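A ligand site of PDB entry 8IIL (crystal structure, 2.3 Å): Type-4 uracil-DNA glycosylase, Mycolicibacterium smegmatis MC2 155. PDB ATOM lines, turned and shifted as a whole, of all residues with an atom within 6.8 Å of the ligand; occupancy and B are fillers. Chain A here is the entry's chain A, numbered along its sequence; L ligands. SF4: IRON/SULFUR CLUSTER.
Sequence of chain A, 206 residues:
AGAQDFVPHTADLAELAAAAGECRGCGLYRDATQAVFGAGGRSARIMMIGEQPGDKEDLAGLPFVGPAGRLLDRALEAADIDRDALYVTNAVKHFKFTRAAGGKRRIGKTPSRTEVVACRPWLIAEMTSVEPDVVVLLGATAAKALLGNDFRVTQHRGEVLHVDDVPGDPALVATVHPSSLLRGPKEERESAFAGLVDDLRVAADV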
ATOM      1  N   GLY A   2       1.856 -19.649  -3.939  1.00  0.00           N
ATOM      2  CA  GLY A   2       1.126 -18.511  -4.484  1.00  0.00           C
ATOM      3  C   GLY A   2       0.936 -17.375  -3.493  1.00  0.00           C
ATOM      4  O   GLY A   2       1.892 -16.875  -2.874  1.00  0.00           O
ATOM      5  N   ALA A   3      -0.327 -16.972  -3.302  1.00  0.00           N
ATOM      6  CA  ALA A   3      -0.710 -15.830  -2.476  1.00  0.00           C
ATOM      7  C   ALA A   3      -0.758 -16.170  -0.990  1.00  0.00           C
ATOM      8  O   ALA A   3      -1.164 -15.322  -0.184  1.00  0.00           O
ATOM      9  CB  ALA A   3      -2.065 -15.273  -2.921  1.00  0.00           C
ATOM     10  N   PHE A   6       0.861 -13.909   1.498  1.00  0.00           N
ATOM     11  CA  PHE A   6       0.361 -12.542   1.474  1.00  0.00           C
ATOM     12  C   PHE A   6      -0.965 -12.408   2.202  1.00  0.00           C
ATOM     13  O   PHE A   6      -1.306 -11.297   2.644  1.00  0.00           O
ATOM     14  CB  PHE A   6       0.268 -12.078   0.017  1.00  0.00           C
ATOM     15  CG  PHE A   6       1.598 -11.963  -0.670  1.00  0.00           C
ATOM     16  CD1 PHE A   6       2.427 -10.875  -0.422  1.00  0.00           C
ATOM     17  CD2 PHE A   6       2.056 -12.961  -1.512  1.00  0.00           C
ATOM     18  CE1 PHE A   6       3.674 -10.765  -1.038  1.00  0.00           C
ATOM     19  CE2 PHE A   6       3.306 -12.854  -2.141  1.00  0.00           C
ATOM     20  CZ  PHE A   6       4.117 -11.750  -1.894  1.00  0.00           C
ATOM     21  N   ALA A  20      -4.507  -7.758  -0.218  1.00  0.00           N
ATOM     22  CA  ALA A  20      -4.524  -8.142  -1.644  1.00  0.00           C
ATOM     23  C   ALA A  20      -3.853  -7.067  -2.507  1.00  0.00           C
ATOM     24  O   ALA A  20      -3.290  -7.417  -3.539  1.00  0.00           O
ATOM     25  CB  ALA A  20      -5.905  -8.511  -2.092  1.00  0.00           C
ATOM     26  N   GLY A  21      -3.876  -5.804  -2.071  1.00  0.00           N
ATOM     27  CA  GLY A  21      -3.179  -4.727  -2.787  1.00  0.00           C
ATOM     28  C   GLY A  21      -1.669  -4.857  -2.835  1.00  0.00           C
ATOM     29  O   GLY A  21      -1.084  -4.283  -3.745  1.00  0.00           O
ATOM     30  N   GLU A  22      -1.050  -5.571  -1.899  1.00  0.00           N
ATOM     31  CA  GLU A  22       0.417  -5.808  -1.902  1.00  0.00           C
ATOM     32  C   GLU A  22       0.772  -7.217  -2.385  1.00  0.00           C
ATOM     33  O   GLU A  22       1.953  -7.547  -2.410  1.00  0.00           O
ATOM     34  CB  GLU A  22       0.970  -5.685  -0.495  1.00  0.00           C
ATOM     35  N   CYS A  23      -0.227  -8.013  -2.745  1.00  0.00           N
ATOM     36  CA  CYS A  23      -0.008  -9.435  -3.114  1.00  0.00           C
ATOM     37  C   CYS A  23       0.869  -9.602  -4.369  1.00  0.00           C
ATOM     38  O   CYS A  23       0.690  -8.851  -5.316  1.00  0.00           O
ATOM     39  CB  CYS A  23      -1.323 -10.197  -3.221  1.00  0.00           C
ATOM     40  SG  CYS A  23      -1.170 -11.939  -3.667  1.00  0.00           S
ATOM     41  N   ARG A  24       1.795 -10.561  -4.325  1.00  0.00           N
ATOM     42  CA  ARG A  24       2.693 -10.866  -5.468  1.00  0.00           C
ATOM     43  C   ARG A  24       2.570 -12.371  -5.712  1.00  0.00           C
ATOM     44  O   ARG A  24       3.521 -12.942  -6.270  1.00  0.00           O
ATOM     45  CB  ARG A  24       4.099 -10.327  -5.179  1.00  0.00           C
ATOM     46  CG  ARG A  24       4.155  -8.813  -5.012  1.00  0.00           C
ATOM     47  CD  ARG A  24       5.524  -8.206  -4.769  1.00  0.00           C
ATOM     48  NE  ARG A  24       6.425  -9.058  -4.012  1.00  0.00           N
ATOM     49  CZ  ARG A  24       6.558  -9.025  -2.689  1.00  0.00           C
ATOM     50  NH1 ARG A  24       5.834  -8.184  -1.976  1.00  0.00           N
ATOM     51  NH2 ARG A  24       7.401  -9.841  -2.094  1.00  0.00           N
ATOM     52  N   GLY A  25       1.445 -12.968  -5.322  1.00  0.00           N
ATOM     53  CA  GLY A  25       1.170 -14.420  -5.463  1.00  0.00           C
ATOM     54  C   GLY A  25       1.438 -14.961  -6.839  1.00  0.00           C
ATOM     55  O   GLY A  25       1.939 -16.096  -6.890  1.00  0.00           O
ATOM     56  N   CYS A  26       1.150 -14.212  -7.886  1.00  0.00           N
ATOM     57  CA  CYS A  26       1.470 -14.575  -9.298  1.00  0.00           C
ATOM     58  C   CYS A  26       1.954 -13.288  -9.999  1.00  0.00           C
ATOM     59  O   CYS A  26       2.059 -12.286  -9.334  1.00  0.00           O
ATOM     60  CB  CYS A  26       0.274 -15.192 -10.011  1.00  0.00           C
ATOM     61  SG  CYS A  26      -1.088 -14.054 -10.353  1.00  0.00           S
ATOM     62  N   GLY A  27       2.182 -13.330 -11.312  1.00  0.00           N
ATOM     63  CA  GLY A  27       2.669 -12.144 -12.042  1.00  0.00           C
ATOM     64  C   GLY A  27       1.657 -11.057 -12.403  1.00  0.00           C
ATOM     65  O   GLY A  27       2.106  -9.975 -12.709  1.00  0.00           O
ATOM     66  N   LEU A  28       0.359 -11.319 -12.329  1.00  0.00           N
ATOM     67  CA  LEU A  28      -0.704 -10.359 -12.791  1.00  0.00           C
ATOM     68  C   LEU A  28      -0.739  -8.986 -12.079  1.00  0.00           C
ATOM     69  O   LEU A  28      -1.310  -8.086 -12.667  1.00  0.00           O
ATOM     70  CB  LEU A  28      -2.068 -11.062 -12.751  1.00  0.00           C
ATOM     71  CG  LEU A  28      -2.158 -12.380 -13.505  1.00  0.00           C
ATOM     72  CD1 LEU A  28      -3.554 -12.975 -13.386  1.00  0.00           C
ATOM     73  CD2 LEU A  28      -1.766 -12.199 -14.965  1.00  0.00           C
ATOM     74  N   TYR A  29      -0.216  -8.840 -10.862  1.00  0.00           N
ATOM     75  CA  TYR A  29      -0.131  -7.546 -10.141  1.00  0.00           C
ATOM     76  C   TYR A  29       0.719  -6.526 -10.913  1.00  0.00           C
ATOM     77  O   TYR A  29       0.502  -5.339 -10.691  1.00  0.00           O
ATOM     78  CB  TYR A  29       0.469  -7.724  -8.737  1.00  0.00           C
ATOM     79  CG  TYR A  29       1.972  -7.872  -8.700  1.00  0.00           C
ATOM     80  CD1 TYR A  29       2.574  -9.085  -8.984  1.00  0.00           C
ATOM     81  CD2 TYR A  29       2.785  -6.800  -8.385  1.00  0.00           C
ATOM     82  CE1 TYR A  29       3.950  -9.229  -8.978  1.00  0.00           C
ATOM     83  CE2 TYR A  29       4.164  -6.922  -8.368  1.00  0.00           C
ATOM     84  CZ  TYR A  29       4.745  -8.141  -8.664  1.00  0.00           C
ATOM     85  OH  TYR A  29       6.103  -8.255  -8.645  1.00  0.00           O
ATOM     86  N   ARG A  30       1.599  -6.979 -11.820  1.00  0.00           N
ATOM     87  CA  ARG A  30       2.552  -6.087 -12.517  1.00  0.00           C
ATOM     88  C   ARG A  30       1.889  -5.150 -13.536  1.00  0.00           C
ATOM     89  O   ARG A  30       2.205  -3.973 -13.508  1.00  0.00           O
ATOM     90  CB  ARG A  30       3.697  -6.907 -13.116  1.00  0.00           C
ATOM     91  CG  ARG A  30       4.794  -7.234 -12.121  1.00  0.00           C
ATOM     92  CD  ARG A  30       5.868  -8.167 -12.635  1.00  0.00           C
ATOM     93  NE  ARG A  30       5.639  -9.552 -12.247  1.00  0.00           N
ATOM     94  CZ  ARG A  30       6.540 -10.310 -11.638  1.00  0.00           C
ATOM     95  NH1 ARG A  30       7.732  -9.819 -11.342  1.00  0.00           N
ATOM     96  NH2 ARG A  30       6.253 -11.559 -11.315  1.00  0.00           N
ATOM     97  N   ALA A  35      -5.372  -4.273  -7.109  1.00  0.00           N
ATOM     98  CA  ALA A  35      -6.118  -5.502  -6.786  1.00  0.00           C
ATOM     99  C   ALA A  35      -7.604  -5.172  -6.711  1.00  0.00           C
ATOM    100  O   ALA A  35      -7.954  -4.112  -6.208  1.00  0.00           O
ATOM    101  CB  ALA A  35      -5.607  -6.131  -5.530  1.00  0.00           C
ATOM    102  N   ALA A  91     -12.174 -15.158  -9.057  1.00  0.00           N
ATOM    103  CA  ALA A  91     -11.190 -16.230  -8.796  1.00  0.00           C
ATOM    104  C   ALA A  91      -9.787 -15.634  -8.758  1.00  0.00           C
ATOM    105  O   ALA A  91      -9.029 -16.043  -7.904  1.00  0.00           O
ATOM    106  CB  ALA A  91     -11.357 -17.246  -9.888  1.00  0.00           C
ATOM    107  N   VAL A  92      -9.464 -14.747  -9.702  1.00  0.00           N
ATOM    108  CA  VAL A  92      -8.183 -14.002  -9.704  1.00  0.00           C
ATOM    109  C   VAL A  92      -8.533 -12.521  -9.430  1.00  0.00           C
ATOM    110  O   VAL A  92      -9.617 -12.108  -9.840  1.00  0.00           O
ATOM    111  CB  VAL A  92      -7.365 -14.302 -10.986  1.00  0.00           C
ATOM    112  CG1 VAL A  92      -7.453 -15.765 -11.365  1.00  0.00           C
ATOM    113  CG2 VAL A  92      -7.676 -13.405 -12.153  1.00  0.00           C
ATOM    114  N   LYS A  93      -7.700 -11.782  -8.686  1.00  0.00           N
ATOM    115  CA  LYS A  93      -8.051 -10.401  -8.241  1.00  0.00           C
ATOM    116  C   LYS A  93      -7.386  -9.314  -9.101  1.00  0.00           C
ATOM    117  O   LYS A  93      -7.715  -8.161  -8.918  1.00  0.00           O
ATOM    118  CB  LYS A  93      -7.672 -10.242  -6.756  1.00  0.00           C
ATOM    119  CG  LYS A  93      -8.233 -11.283  -5.793  1.00  0.00           C
ATOM    120  CD  LYS A  93      -9.719 -11.240  -5.647  1.00  0.00           C
ATOM    121  CE  LYS A  93     -10.199 -11.877  -4.371  1.00  0.00           C
ATOM    122  NZ  LYS A  93     -10.917 -13.139  -4.620  1.00  0.00           N
ATOM    123  N   HIS A  94      -6.456  -9.722  -9.954  1.00  0.00           N
ATOM    124  CA  HIS A  94      -5.725  -8.776 -10.833  1.00  0.00           C
ATOM    125  C   HIS A  94      -6.119  -9.011 -12.289  1.00  0.00           C
ATOM    126  O   HIS A  94      -6.106 -10.164 -12.716  1.00  0.00           O
ATOM    127  CB  HIS A  94      -4.220  -8.835 -10.563  1.00  0.00           C
ATOM    128  CG  HIS A  94      -3.719  -7.901  -9.517  1.00  0.00           C
ATOM    129  ND1 HIS A  94      -3.321  -8.327  -8.281  1.00  0.00           N
ATOM    130  CD2 HIS A  94      -3.541  -6.568  -9.519  1.00  0.00           C
ATOM    131  CE1 HIS A  94      -2.921  -7.306  -7.566  1.00  0.00           C
ATOM    132  NE2 HIS A  94      -3.046  -6.222  -8.302  1.00  0.00           N
ATOM    133  N   PHE A  95      -6.422  -7.954 -13.016  1.00  0.00           N
ATOM    134  CA  PHE A  95      -6.801  -8.019 -14.440  1.00  0.00           C
ATOM    135  C   PHE A  95      -5.666  -8.572 -15.325  1.00  0.00           C
ATOM    136  O   PHE A  95      -4.591  -7.984 -15.398  1.00  0.00           O
ATOM    137  CB  PHE A  95      -7.244  -6.632 -14.902  1.00  0.00           C
ATOM    138  CG  PHE A  95      -7.793  -6.458 -16.301  1.00  0.00           C
ATOM    139  CD1 PHE A  95      -8.514  -7.449 -16.932  1.00  0.00           C
ATOM    140  CD2 PHE A  95      -7.602  -5.264 -16.974  1.00  0.00           C
ATOM    141  CE1 PHE A  95      -9.030  -7.266 -18.200  1.00  0.00           C
ATOM    142  CE2 PHE A  95      -8.107  -5.075 -18.248  1.00  0.00           C
ATOM    143  CZ  PHE A  95      -8.829  -6.072 -18.856  1.00  0.00           C
ATOM    144  N   GLU A 115      -2.640 -19.486 -12.127  1.00  0.00           N
ATOM    145  CA  GLU A 115      -3.008 -18.180 -11.512  1.00  0.00           C
ATOM    146  C   GLU A 115      -4.263 -18.322 -10.639  1.00  0.00           C
ATOM    147  O   GLU A 115      -4.300 -17.675  -9.613  1.00  0.00           O
ATOM    148  CB  GLU A 115      -3.097 -17.083 -12.570  1.00  0.00           C
ATOM    149  CG  GLU A 115      -1.801 -16.804 -13.302  1.00  0.00           C
ATOM    150  CD  GLU A 115      -2.001 -16.243 -14.694  1.00  0.00           C
ATOM    151  OE1 GLU A 115      -3.070 -16.477 -15.272  1.00  0.00           O
ATOM    152  OE2 GLU A 115      -1.097 -15.570 -15.197  1.00  0.00           O
ATOM    153  N   VAL A 117      -5.145 -21.085  -8.979  1.00  0.00           N
ATOM    154  CA  VAL A 117      -4.604 -21.762  -7.765  1.00  0.00           C
ATOM    155  C   VAL A 117      -3.785 -20.778  -6.902  1.00  0.00           C
ATOM    156  O   VAL A 117      -3.954 -20.803  -5.694  1.00  0.00           O
ATOM    157  CB  VAL A 117      -3.848 -23.068  -8.119  1.00  0.00           C
ATOM    158  CG1 VAL A 117      -3.070 -23.647  -6.947  1.00  0.00           C
ATOM    159  CG2 VAL A 117      -4.781 -24.110  -8.699  1.00  0.00           C
ATOM    160  N   ALA A 118      -3.017 -19.900  -7.527  1.00  0.00           N
ATOM    161  CA  ALA A 118      -2.226 -18.884  -6.796  1.00  0.00           C
ATOM    162  C   ALA A 118      -3.146 -17.931  -6.035  1.00  0.00           C
ATOM    163  O   ALA A 118      -2.842 -17.682  -4.885  1.00  0.00           O
ATOM    164  CB  ALA A 118      -1.301 -18.146  -7.725  1.00  0.00           C
ATOM    165  N   CYS A 119      -4.281 -17.574  -6.637  1.00  0.00           N
ATOM    166  CA  CYS A 119      -5.230 -16.614  -6.032  1.00  0.00           C
ATOM    167  C   CYS A 119      -6.229 -17.281  -5.069  1.00  0.00           C
ATOM    168  O   CYS A 119      -6.775 -16.565  -4.243  1.00  0.00           O
ATOM    169  CB  CYS A 119      -5.954 -15.895  -7.150  1.00  0.00           C
ATOM    170  SG  CYS A 119      -6.478 -14.264  -6.608  1.00  0.00           S
ATOM    171  N   ARG A 120      -6.454 -18.579  -5.212  1.00  0.00           N
ATOM    172  CA  ARG A 120      -7.440 -19.346  -4.388  1.00  0.00           C
ATOM    173  C   ARG A 120      -7.329 -19.033  -2.880  1.00  0.00           C
ATOM    174  O   ARG A 120      -8.373 -18.912  -2.271  1.00  0.00           O
ATOM    175  CB  ARG A 120      -7.510 -20.821  -4.811  1.00  0.00           C
ATOM    176  CG  ARG A 120      -8.725 -21.558  -4.269  1.00  0.00           C
ATOM    177  CD  ARG A 120      -8.903 -22.933  -4.882  1.00  0.00           C
ATOM    178  NE  ARG A 120      -7.694 -23.736  -4.823  1.00  0.00           N
ATOM    179  CZ  ARG A 120      -7.513 -24.855  -5.508  1.00  0.00           C
ATOM    180  NH1 ARG A 120      -8.463 -25.317  -6.290  1.00  0.00           N
ATOM    181  NH2 ARG A 120      -6.371 -25.512  -5.393  1.00  0.00           N
ATOM    182  N   TRP A 122      -7.057 -16.239  -1.328  1.00  0.00           N
ATOM    183  CA  TRP A 122      -7.917 -15.045  -1.091  1.00  0.00           C
ATOM    184  C   TRP A 122      -9.394 -15.453  -1.092  1.00  0.00           C
ATOM    185  O   TRP A 122     -10.104 -14.953  -0.224  1.00  0.00           O
ATOM    186  CB  TRP A 122      -7.649 -13.953  -2.125  1.00  0.00           C
ATOM    187  CG  TRP A 122      -6.308 -13.321  -2.050  1.00  0.00           C
ATOM    188  CD1 TRP A 122      -5.324 -13.378  -2.992  1.00  0.00           C
ATOM    189  CD2 TRP A 122      -5.781 -12.527  -0.965  1.00  0.00           C
ATOM    190  NE1 TRP A 122      -4.227 -12.678  -2.565  1.00  0.00           N
ATOM    191  CE2 TRP A 122      -4.474 -12.154  -1.329  1.00  0.00           C
ATOM    192  CE3 TRP A 122      -6.285 -12.112   0.267  1.00  0.00           C
ATOM    193  CZ2 TRP A 122      -3.663 -11.394  -0.491  1.00  0.00           C
ATOM    194  CZ3 TRP A 122      -5.498 -11.348   1.084  1.00  0.00           C
ATOM    195  CH2 TRP A 122      -4.207 -10.993   0.705  1.00  0.00           C
HETATM  196 FE1  SF4 L   1      -4.349 -13.016  -7.027  1.00  0.00          FE
HETATM  197 FE2  SF4 L   1      -1.904 -13.069  -8.482  1.00  0.00          FE
HETATM  198 FE3  SF4 L   1      -1.950 -12.117  -5.834  1.00  0.00          FE
HETATM  199 FE4  SF4 L   1      -3.152 -10.617  -7.840  1.00  0.00          FE
HETATM  200  S1  SF4 L   1      -0.911 -11.166  -7.632  1.00  0.00           S
HETATM  201  S2  SF4 L   1      -4.024 -11.105  -5.789  1.00  0.00           S
HETATM  202  S3  SF4 L   1      -3.981 -12.309  -9.184  1.00  0.00           S
HETATM  203  S4  SF4 L   1      -2.422 -14.243  -6.566  1.00  0.00           S
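Residues that only touch the ligand: Ala 3, Tyr 29 and Ala 118.
Of the 26 residues printed, 10 come within 4 Å of the ligand.
Along chain A the residues within 4 Å of the ligand span positions 3 to 122.
The nearest printed residue that does not touch the ligand is Arg 24 (4.2 Å).
The side-chain sulfur of Cys 26 sits close to the backbone NH of Leu 28, at 3.7 Å.
The side-chain sulfur of Cys 23 sits close to the backbone NH of Gly 25, 3.3 Å away.
SG of Cys 23 sits close to NE1 of Trp 122, 3.3 Å away.
The backbone NH (N) of Ala 35 sits at hydrogen-bond distance from a ring nitrogen (NE2) of His 94, 3.3 Å away.
SG of Cys 119 sits close to N of Lys 93 (3.5 Å).
The side-chain sulfur of Cys 119 lies close to the backbone carbonyl oxygen of Ala 91 (3.4 Å).
N of Ala 3 is in hydrogen-bond range of O of Ala 118, 3.1 Å away.
N of Cys 26 lies close to S1 of the ligand (3.7 Å).
SG of Cys 26 is bound to FE2 of the ligand, 2.3 Å away.
SG of Cys 23 binds FE3 of the ligand.
The backbone NH (N) of His 94 sits close to a sulfur (S3) of the ligand (3.7 Å).
A ring nitrogen (ND1) of His 94 is bound to an iron atom (FE4) of the ligand, at 2.3 Å.
The side-chain sulfur (SG) of Cys 119 is bound to an iron atom (FE1) of the ligand (2.5 Å).
A sulfur (S1) of the ligand sits close to the backbone NH (N) of Gly 25, at 3.8 Å.
The indole nitrogen (NE1) of Trp 122 sits close to a sulfur (S2) of the ligand.
The backbone NH of Lys 93 lies close to a sulfur (S3) of the ligand (3.8 Å).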
